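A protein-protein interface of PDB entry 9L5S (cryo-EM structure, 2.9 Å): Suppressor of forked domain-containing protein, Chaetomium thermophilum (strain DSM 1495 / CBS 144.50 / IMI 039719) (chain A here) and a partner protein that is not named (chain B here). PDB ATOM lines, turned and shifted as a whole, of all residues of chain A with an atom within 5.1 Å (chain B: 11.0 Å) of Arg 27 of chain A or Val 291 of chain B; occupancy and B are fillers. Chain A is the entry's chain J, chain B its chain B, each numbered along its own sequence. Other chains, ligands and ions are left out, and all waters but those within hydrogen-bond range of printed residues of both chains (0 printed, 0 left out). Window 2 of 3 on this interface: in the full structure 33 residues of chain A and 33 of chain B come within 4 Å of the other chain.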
ATOM      1  N   GLU A  23     -12.677   6.028  10.733  1.00  0.00           N
ATOM      2  CA  GLU A  23     -12.275   7.174  11.542  1.00  0.00           C
ATOM      3  C   GLU A  23     -13.380   8.221  11.614  1.00  0.00           C
ATOM      4  O   GLU A  23     -13.431   8.991  12.576  1.00  0.00           O
ATOM      5  CB  GLU A  23     -10.973   7.807  11.023  1.00  0.00           C
ATOM      6  CG  GLU A  23      -9.798   6.858  10.693  1.00  0.00           C
ATOM      7  CD  GLU A  23      -9.961   6.055   9.410  1.00  0.00           C
ATOM      8  OE1 GLU A  23     -10.979   6.234   8.710  1.00  0.00           O
ATOM      9  OE2 GLU A  23      -9.071   5.234   9.111  1.00  0.00           O
ATOM     10  N   GLN A  24     -14.276   8.254  10.624  1.00  0.00           N
ATOM     11  CA  GLN A  24     -15.486   9.064  10.743  1.00  0.00           C
ATOM     12  C   GLN A  24     -16.341   8.596  11.918  1.00  0.00           C
ATOM     13  O   GLN A  24     -16.787   9.409  12.743  1.00  0.00           O
ATOM     14  CB  GLN A  24     -16.285   9.002   9.441  1.00  0.00           C
ATOM     15  CG  GLN A  24     -15.526   9.476   8.214  1.00  0.00           C
ATOM     16  CD  GLN A  24     -16.431   9.737   7.025  1.00  0.00           C
ATOM     17  OE1 GLN A  24     -17.655   9.661   7.132  1.00  0.00           O
ATOM     18  NE2 GLN A  24     -15.831  10.052   5.883  1.00  0.00           N
ATOM     19  N   LEU A  25     -16.565   7.278  12.013  1.00  0.00           N
ATOM     20  CA  LEU A  25     -17.294   6.714  13.145  1.00  0.00           C
ATOM     21  C   LEU A  25     -16.590   7.024  14.457  1.00  0.00           C
ATOM     22  O   LEU A  25     -17.243   7.281  15.473  1.00  0.00           O
ATOM     23  CB  LEU A  25     -17.458   5.201  12.983  1.00  0.00           C
ATOM     24  CG  LEU A  25     -18.584   4.593  12.135  1.00  0.00           C
ATOM     25  CD1 LEU A  25     -19.940   4.931  12.735  1.00  0.00           C
ATOM     26  CD2 LEU A  25     -18.525   4.991  10.671  1.00  0.00           C
ATOM     27  N   LEU A  26     -15.257   7.044  14.442  1.00  0.00           N
ATOM     28  CA  LEU A  26     -14.514   7.443  15.633  1.00  0.00           C
ATOM     29  C   LEU A  26     -14.727   8.921  15.963  1.00  0.00           C
ATOM     30  O   LEU A  26     -14.782   9.292  17.143  1.00  0.00           O
ATOM     31  CB  LEU A  26     -13.033   7.126  15.442  1.00  0.00           C
ATOM     32  CG  LEU A  26     -12.743   5.633  15.615  1.00  0.00           C
ATOM     33  CD1 LEU A  26     -11.287   5.307  15.344  1.00  0.00           C
ATOM     34  CD2 LEU A  26     -13.139   5.186  17.015  1.00  0.00           C
ATOM     35  N   ARG A  27     -14.853   9.778  14.941  1.00  0.00           N
ATOM     36  CA  ARG A  27     -15.069  11.202  15.196  1.00  0.00           C
ATOM     37  C   ARG A  27     -16.437  11.489  15.807  1.00  0.00           C
ATOM     38  O   ARG A  27     -16.521  12.278  16.756  1.00  0.00           O
ATOM     39  CB  ARG A  27     -14.901  12.039  13.925  1.00  0.00           C
ATOM     40  CG  ARG A  27     -13.481  12.099  13.391  1.00  0.00           C
ATOM     41  CD  ARG A  27     -13.368  13.017  12.181  1.00  0.00           C
ATOM     42  NE  ARG A  27     -14.041  12.513  10.991  1.00  0.00           N
ATOM     43  CZ  ARG A  27     -15.110  13.085  10.454  1.00  0.00           C
ATOM     44  NH1 ARG A  27     -15.652  14.169  10.982  1.00  0.00           N
ATOM     45  NH2 ARG A  27     -15.642  12.563   9.353  1.00  0.00           N
ATOM     46  N   GLU A  28     -17.516  10.885  15.297  1.00  0.00           N
ATOM     47  CA  GLU A  28     -18.754  11.032  16.071  1.00  0.00           C
ATOM     48  C   GLU A  28     -18.833  10.115  17.291  1.00  0.00           C
ATOM     49  O   GLU A  28     -19.785  10.243  18.068  1.00  0.00           O
ATOM     50  CB  GLU A  28     -20.055  10.865  15.256  1.00  0.00           C
ATOM     51  CG  GLU A  28     -20.396  11.950  14.211  1.00  0.00           C
ATOM     52  CD  GLU A  28     -19.740  11.795  12.871  1.00  0.00           C
ATOM     53  OE1 GLU A  28     -19.046  10.800  12.667  1.00  0.00           O
ATOM     54  OE2 GLU A  28     -19.929  12.675  12.006  1.00  0.00           O
ATOM     55  N   ALA A  29     -17.876   9.208  17.490  1.00  0.00           N
ATOM     56  CA  ALA A  29     -17.816   8.492  18.760  1.00  0.00           C
ATOM     57  C   ALA A  29     -17.210   9.354  19.861  1.00  0.00           C
ATOM     58  O   ALA A  29     -17.626   9.261  21.021  1.00  0.00           O
ATOM     59  CB  ALA A  29     -17.019   7.197  18.596  1.00  0.00           C
ATOM     60  N   VAL A  30     -16.223  10.185  19.518  1.00  0.00           N
ATOM     61  CA  VAL A  30     -15.577  11.037  20.516  1.00  0.00           C
ATOM     62  C   VAL A  30     -16.528  12.134  20.984  1.00  0.00           C
ATOM     63  O   VAL A  30     -16.679  12.378  22.188  1.00  0.00           O
ATOM     64  CB  VAL A  30     -14.274  11.629  19.948  1.00  0.00           C
ATOM     65  CG1 VAL A  30     -13.732  12.726  20.856  1.00  0.00           C
ATOM     66  CG2 VAL A  30     -13.238  10.543  19.765  1.00  0.00           C
ATOM     67  N   ASP A  31     -17.202  12.795  20.040  1.00  0.00           N
ATOM     68  CA  ASP A  31     -17.977  13.992  20.345  1.00  0.00           C
ATOM     69  C   ASP A  31     -19.276  13.701  21.087  1.00  0.00           C
ATOM     70  O   ASP A  31     -19.893  14.639  21.603  1.00  0.00           O
ATOM     71  CB  ASP A  31     -18.284  14.751  19.054  1.00  0.00           C
ATOM     72  CG  ASP A  31     -17.029  15.184  18.322  1.00  0.00           C
ATOM     73  OD1 ASP A  31     -15.971  15.307  18.974  1.00  0.00           O
ATOM     74  OD2 ASP A  31     -17.100  15.400  17.094  1.00  0.00           O
ATOM     75  N   SER B 284      -1.254  19.077  25.158  1.00  0.00           N
ATOM     76  CA  SER B 284      -1.968  17.820  24.984  1.00  0.00           C
ATOM     77  C   SER B 284      -3.408  18.018  24.534  1.00  0.00           C
ATOM     78  O   SER B 284      -4.044  17.048  24.106  1.00  0.00           O
ATOM     79  CB  SER B 284      -1.947  17.015  26.286  1.00  0.00           C
ATOM     80  OG  SER B 284      -2.810  17.587  27.253  1.00  0.00           O
ATOM     81  N   GLU B 286      -4.473  19.509  21.876  1.00  0.00           N
ATOM     82  CA  GLU B 286      -4.559  19.774  20.444  1.00  0.00           C
ATOM     83  C   GLU B 286      -4.882  18.494  19.681  1.00  0.00           C
ATOM     84  O   GLU B 286      -4.268  17.449  19.920  1.00  0.00           O
ATOM     85  CB  GLU B 286      -3.252  20.378  19.928  1.00  0.00           C
ATOM     86  CG  GLU B 286      -2.918  21.738  20.518  1.00  0.00           C
ATOM     87  CD  GLU B 286      -4.127  22.649  20.602  1.00  0.00           C
ATOM     88  OE1 GLU B 286      -4.592  23.122  19.544  1.00  0.00           O
ATOM     89  OE2 GLU B 286      -4.611  22.895  21.727  1.00  0.00           O
ATOM     90  N   GLU B 287      -5.845  18.584  18.765  1.00  0.00           N
ATOM     91  CA  GLU B 287      -6.265  17.453  17.934  1.00  0.00           C
ATOM     92  C   GLU B 287      -5.539  17.398  16.590  1.00  0.00           C
ATOM     93  O   GLU B 287      -6.162  17.253  15.534  1.00  0.00           O
ATOM     94  CB  GLU B 287      -7.781  17.500  17.745  1.00  0.00           C
ATOM     95  CG  GLU B 287      -8.343  18.818  17.197  1.00  0.00           C
ATOM     96  CD  GLU B 287      -8.759  19.784  18.291  1.00  0.00           C
ATOM     97  OE1 GLU B 287      -8.385  19.561  19.461  1.00  0.00           O
ATOM     98  OE2 GLU B 287      -9.463  20.768  17.979  1.00  0.00           O
ATOM     99  N   HIS B 288      -4.210  17.468  16.598  1.00  0.00           N
ATOM    100  CA  HIS B 288      -3.428  17.433  15.363  1.00  0.00           C
ATOM    101  C   HIS B 288      -3.078  15.986  15.043  1.00  0.00           C
ATOM    102  O   HIS B 288      -2.322  15.340  15.772  1.00  0.00           O
ATOM    103  CB  HIS B 288      -2.174  18.289  15.496  1.00  0.00           C
ATOM    104  CG  HIS B 288      -1.355  18.363  14.244  1.00  0.00           C
ATOM    105  ND1 HIS B 288      -0.008  18.655  14.252  1.00  0.00           N
ATOM    106  CD2 HIS B 288      -1.694  18.189  12.944  1.00  0.00           C
ATOM    107  CE1 HIS B 288       0.449  18.653  13.013  1.00  0.00           C
ATOM    108  NE2 HIS B 288      -0.554  18.373  12.200  1.00  0.00           N
ATOM    109  N   GLY B 289      -3.630  15.471  13.947  1.00  0.00           N
ATOM    110  CA  GLY B 289      -3.344  14.139  13.465  1.00  0.00           C
ATOM    111  C   GLY B 289      -4.604  13.316  13.353  1.00  0.00           C
ATOM    112  O   GLY B 289      -5.718  13.797  13.583  1.00  0.00           O
ATOM    113  N   ASP B 290      -4.428  12.048  12.988  1.00  0.00           N
ATOM    114  CA  ASP B 290      -5.552  11.125  12.908  1.00  0.00           C
ATOM    115  C   ASP B 290      -6.045  10.761  14.302  1.00  0.00           C
ATOM    116  O   ASP B 290      -5.254  10.567  15.229  1.00  0.00           O
ATOM    117  CB  ASP B 290      -5.150   9.862  12.148  1.00  0.00           C
ATOM    118  CG  ASP B 290      -6.285   9.299  11.316  1.00  0.00           C
ATOM    119  OD1 ASP B 290      -6.039   8.907  10.157  1.00  0.00           O
ATOM    120  OD2 ASP B 290      -7.426   9.250  11.824  1.00  0.00           O
ATOM    121  N   VAL B 291      -7.362  10.667  14.447  1.00  0.00           N
ATOM    122  CA  VAL B 291      -7.982  10.314  15.719  1.00  0.00           C
ATOM    123  C   VAL B 291      -8.316   8.825  15.717  1.00  0.00           C
ATOM    124  O   VAL B 291      -8.776   8.275  14.708  1.00  0.00           O
ATOM    125  CB  VAL B 291      -9.222  11.192  15.992  1.00  0.00           C
ATOM    126  CG1 VAL B 291     -10.300  11.012  14.926  1.00  0.00           C
ATOM    127  CG2 VAL B 291      -9.791  10.914  17.377  1.00  0.00           C
ATOM    128  N   THR B 292      -8.009   8.153  16.826  1.00  0.00           N
ATOM    129  CA  THR B 292      -8.330   6.740  16.976  1.00  0.00           C
ATOM    130  C   THR B 292      -9.028   6.522  18.315  1.00  0.00           C
ATOM    131  O   THR B 292      -9.903   5.658  18.446  1.00  0.00           O
ATOM    132  CB  THR B 292      -7.059   5.892  16.858  1.00  0.00           C
ATOM    133  OG1 THR B 292      -6.463   6.107  15.573  1.00  0.00           O
ATOM    134  CG2 THR B 292      -7.377   4.409  16.990  1.00  0.00           C
ATOM    135  N   TYR B 293      -8.679   7.349  19.297  1.00  0.00           N
ATOM    136  CA  TYR B 293      -9.144   7.188  20.666  1.00  0.00           C
ATOM    137  C   TYR B 293     -10.631   7.518  20.789  1.00  0.00           C
ATOM    138  O   TYR B 293     -11.292   7.944  19.839  1.00  0.00           O
ATOM    139  CB  TYR B 293      -8.315   8.067  21.601  1.00  0.00           C
ATOM    140  CG  TYR B 293      -8.436   9.562  21.348  1.00  0.00           C
ATOM    141  CD1 TYR B 293      -7.580  10.205  20.461  1.00  0.00           C
ATOM    142  CD2 TYR B 293      -9.387  10.332  22.011  1.00  0.00           C
ATOM    143  CE1 TYR B 293      -7.677  11.565  20.230  1.00  0.00           C
ATOM    144  CE2 TYR B 293      -9.493  11.691  21.784  1.00  0.00           C
ATOM    145  CZ  TYR B 293      -8.637  12.302  20.894  1.00  0.00           C
ATOM    146  OH  TYR B 293      -8.740  13.656  20.668  1.00  0.00           O
ATOM    147  N   ILE B 294     -11.160   7.298  21.992  1.00  0.00           N
ATOM    148  CA  ILE B 294     -12.492   7.774  22.357  1.00  0.00           C
ATOM    149  C   ILE B 294     -12.500   8.597  23.635  1.00  0.00           C
ATOM    150  O   ILE B 294     -13.444   9.379  23.850  1.00  0.00           O
ATOM    151  CB  ILE B 294     -13.488   6.595  22.479  1.00  0.00           C
ATOM    152  CG1 ILE B 294     -13.041   5.619  23.571  1.00  0.00           C
ATOM    153  CG2 ILE B 294     -13.668   5.882  21.143  1.00  0.00           C
ATOM    154  CD1 ILE B 294     -14.101   4.610  23.955  1.00  0.00           C
ATOM    155  N   ASN B 295     -11.490   8.485  24.498  1.00  0.00           N
ATOM    156  CA  ASN B 295     -11.416   9.200  25.766  1.00  0.00           C
ATOM    157  C   ASN B 295     -10.055   9.879  25.881  1.00  0.00           C
ATOM    158  O   ASN B 295      -9.154   9.659  25.066  1.00  0.00           O
ATOM    159  CB  ASN B 295     -11.644   8.254  26.953  1.00  0.00           C
ATOM    160  CG  ASN B 295     -13.099   7.860  27.123  1.00  0.00           C
ATOM    161  OD1 ASN B 295     -13.985   8.408  26.469  1.00  0.00           O
ATOM    162  ND2 ASN B 295     -13.350   6.901  28.004  1.00  0.00           N
ATOM    163  N   GLU B 296      -9.904  10.706  26.921  1.00  0.00           N
ATOM    164  CA  GLU B 296      -8.633  11.389  27.152  1.00  0.00           C
ATOM    165  C   GLU B 296      -7.544  10.409  27.576  1.00  0.00           C
ATOM    166  O   GLU B 296      -6.410  10.478  27.081  1.00  0.00           O
ATOM    167  CB  GLU B 296      -8.814  12.482  28.205  1.00  0.00           C
ATOM    168  CG  GLU B 296      -7.536  13.214  28.584  1.00  0.00           C
ATOM    169  CD  GLU B 296      -6.998  12.782  29.934  1.00  0.00           C
ATOM    170  OE1 GLU B 296      -7.727  12.079  30.666  1.00  0.00           O
ATOM    171  OE2 GLU B 296      -5.850  13.143  30.265  1.00  0.00           O
ATOM    172  N   ASN B 298      -7.607   7.266  26.871  1.00  0.00           N
ATOM    173  CA  ASN B 298      -7.375   6.515  25.642  1.00  0.00           C
ATOM    174  C   ASN B 298      -6.421   7.260  24.716  1.00  0.00           C
ATOM    175  O   ASN B 298      -5.550   6.647  24.091  1.00  0.00           O
ATOM    176  CB  ASN B 298      -8.707   6.247  24.940  1.00  0.00           C
ATOM    177  CG  ASN B 298      -8.609   5.161  23.885  1.00  0.00           C
ATOM    178  OD1 ASN B 298      -7.546   4.584  23.657  1.00  0.00           O
ATOM    179  ND2 ASN B 298      -9.727   4.880  23.230  1.00  0.00           N
ATOM    180  N   LYS B 299      -6.573   8.586  24.620  1.00  0.00           N
ATOM    181  CA  LYS B 299      -5.675   9.392  23.796  1.00  0.00           C
ATOM    182  C   LYS B 299      -4.244   9.337  24.314  1.00  0.00           C
ATOM    183  O   LYS B 299      -3.296   9.186  23.531  1.00  0.00           O
ATOM    184  CB  LYS B 299      -6.173  10.837  23.749  1.00  0.00           C
ATOM    185  CG  LYS B 299      -5.288  11.781  22.952  1.00  0.00           C
ATOM    186  CD  LYS B 299      -5.832  13.201  22.988  1.00  0.00           C
ATOM    187  CE  LYS B 299      -5.166  14.075  21.940  1.00  0.00           C
ATOM    188  NZ  LYS B 299      -6.038  15.212  21.536  1.00  0.00           N
ATOM    189  N   GLN B 300      -4.069   9.443  25.635  1.00  0.00           N
ATOM    190  CA  GLN B 300      -2.730   9.378  26.212  1.00  0.00           C
ATOM    191  C   GLN B 300      -2.111   7.995  26.039  1.00  0.00           C
ATOM    192  O   GLN B 300      -0.915   7.875  25.733  1.00  0.00           O
ATOM    193  CB  GLN B 300      -2.781   9.766  27.688  1.00  0.00           C
ATOM    194  CG  GLN B 300      -3.321  11.163  27.947  1.00  0.00           C
ATOM    195  CD  GLN B 300      -2.617  12.226  27.125  1.00  0.00           C
ATOM    196  OE1 GLN B 300      -1.387  12.279  27.076  1.00  0.00           O
ATOM    197  NE2 GLN B 300      -3.396  13.079  26.469  1.00  0.00           N
ATOM    198  N   ASN B 302      -2.814   5.851  23.625  1.00  0.00           N
ATOM    199  CA  ASN B 302      -2.480   5.685  22.214  1.00  0.00           C
ATOM    200  C   ASN B 302      -1.247   6.491  21.830  1.00  0.00           C
ATOM    201  O   ASN B 302      -0.463   6.052  20.980  1.00  0.00           O
ATOM    202  CB  ASN B 302      -3.672   6.074  21.342  1.00  0.00           C
ATOM    203  CG  ASN B 302      -4.824   5.102  21.474  1.00  0.00           C
ATOM    204  OD1 ASN B 302      -4.644   3.892  21.370  1.00  0.00           O
ATOM    205  ND2 ASN B 302      -6.018   5.629  21.711  1.00  0.00           N
ATOM    206  N   ALA B 303      -1.051   7.661  22.446  1.00  0.00           N
ATOM    207  CA  ALA B 303       0.185   8.409  22.232  1.00  0.00           C
ATOM    208  C   ALA B 303       1.392   7.639  22.754  1.00  0.00           C
ATOM    209  O   ALA B 303       2.450   7.616  22.111  1.00  0.00           O
ATOM    210  CB  ALA B 303       0.093   9.781  22.899  1.00  0.00           C
ATOM    211  N   GLU B 321      -2.166   2.195   5.360  1.00  0.00           N
ATOM    212  CA  GLU B 321      -2.411   3.406   4.583  1.00  0.00           C
ATOM    213  C   GLU B 321      -2.654   3.088   3.114  1.00  0.00           C
ATOM    214  O   GLU B 321      -3.505   3.715   2.472  1.00  0.00           O
ATOM    215  CB  GLU B 321      -1.238   4.376   4.729  1.00  0.00           C
ATOM    216  CG  GLU B 321      -1.446   5.459   5.774  1.00  0.00           C
ATOM    217  CD  GLU B 321      -0.150   6.131   6.180  1.00  0.00           C
ATOM    218  OE1 GLU B 321       0.796   6.142   5.364  1.00  0.00           O
ATOM    219  OE2 GLU B 321      -0.078   6.653   7.313  1.00  0.00           O
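No residue of chain B comes within 4 Å of Gln 24 of chain A. Leu 26 of chain A touches just these residues of chain B: Val 291 (3.9 Å) and Thr 292 (3.4 Å). Arg 27 of chain A touches just one residue of chain B: Val 291. Val 30 of chain A touches two residues of chain B. No residue of chain B comes within 4 Å of Asp 31 of chain A. Of the printed residues of chain A, Asp 290 of chain B touches Glu 23. Of chain A, only Leu 26 (3.9 Å) and Arg 27 (3.7 Å) come within 4 Å of Val 291 of chain B. Printed residues of chain A within 4 Å of Thr 292 of chain B: Leu 26. Of the printed residues of chain A, Tyr 293 of chain B touches Val 30. Of the printed residues of chain A, Ile 294 of chain B touches Val 30 (3.9 Å). Lys 299 of chain B touches none of the printed residues of chain A. The nearest residue of chain B that does not touch Arg 27 of chain A is Tyr 293 of chain B (6.3 Å). The nearest residue of chain A that does not touch Val 291 of chain B is Val 30 of chain A (4.2 Å). The nearest printed residue of chain A that does not touch Asp 290 of chain B is Leu 26 of chain A (6.5 Å).
Of the 18 printed residues of chain B, 5 touch a printed residue of chain A. Printed residues of chain B that touch a printed residue of chain A: Asp 290, Val 291, Thr 292, Tyr 293 and Ile 294. Of the 9 printed residues of chain A, 4 touch a printed residue of chain B. Printed residues of chain A that touch a printed residue of chain B: Glu 23, Leu 26, Arg 27 and Val 30. Hydrophobic or aromatic side chains of chain A that line the printed part of chain B: Leu 26 and Val 30. Along chain A the printed residues that touch a printed residue of chain B span positions 23 to 30.
Glu 23 of chain A touches Asp 290 of chain B. CD1 of Leu 26 of chain A touches O of Val 291 of chain B (3.9 Å). CD1 of Leu 26 of chain A touches O of Thr 292 of chain B, 3.4 Å away. Val 291 of chain B touches Arg 27 of chain A. Tyr 293 of chain B touches Val 30 of chain A. Ile 294 of chain B touches Val 30 of chain A.
OH of Tyr 293 of chain B is in hydrogen-bond range of NZ of Lys 299 of chain B (3.2 Å). N of Ile 294 of chain B sits close to ND2 of Asn 298 of chain B (3.1 Å).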
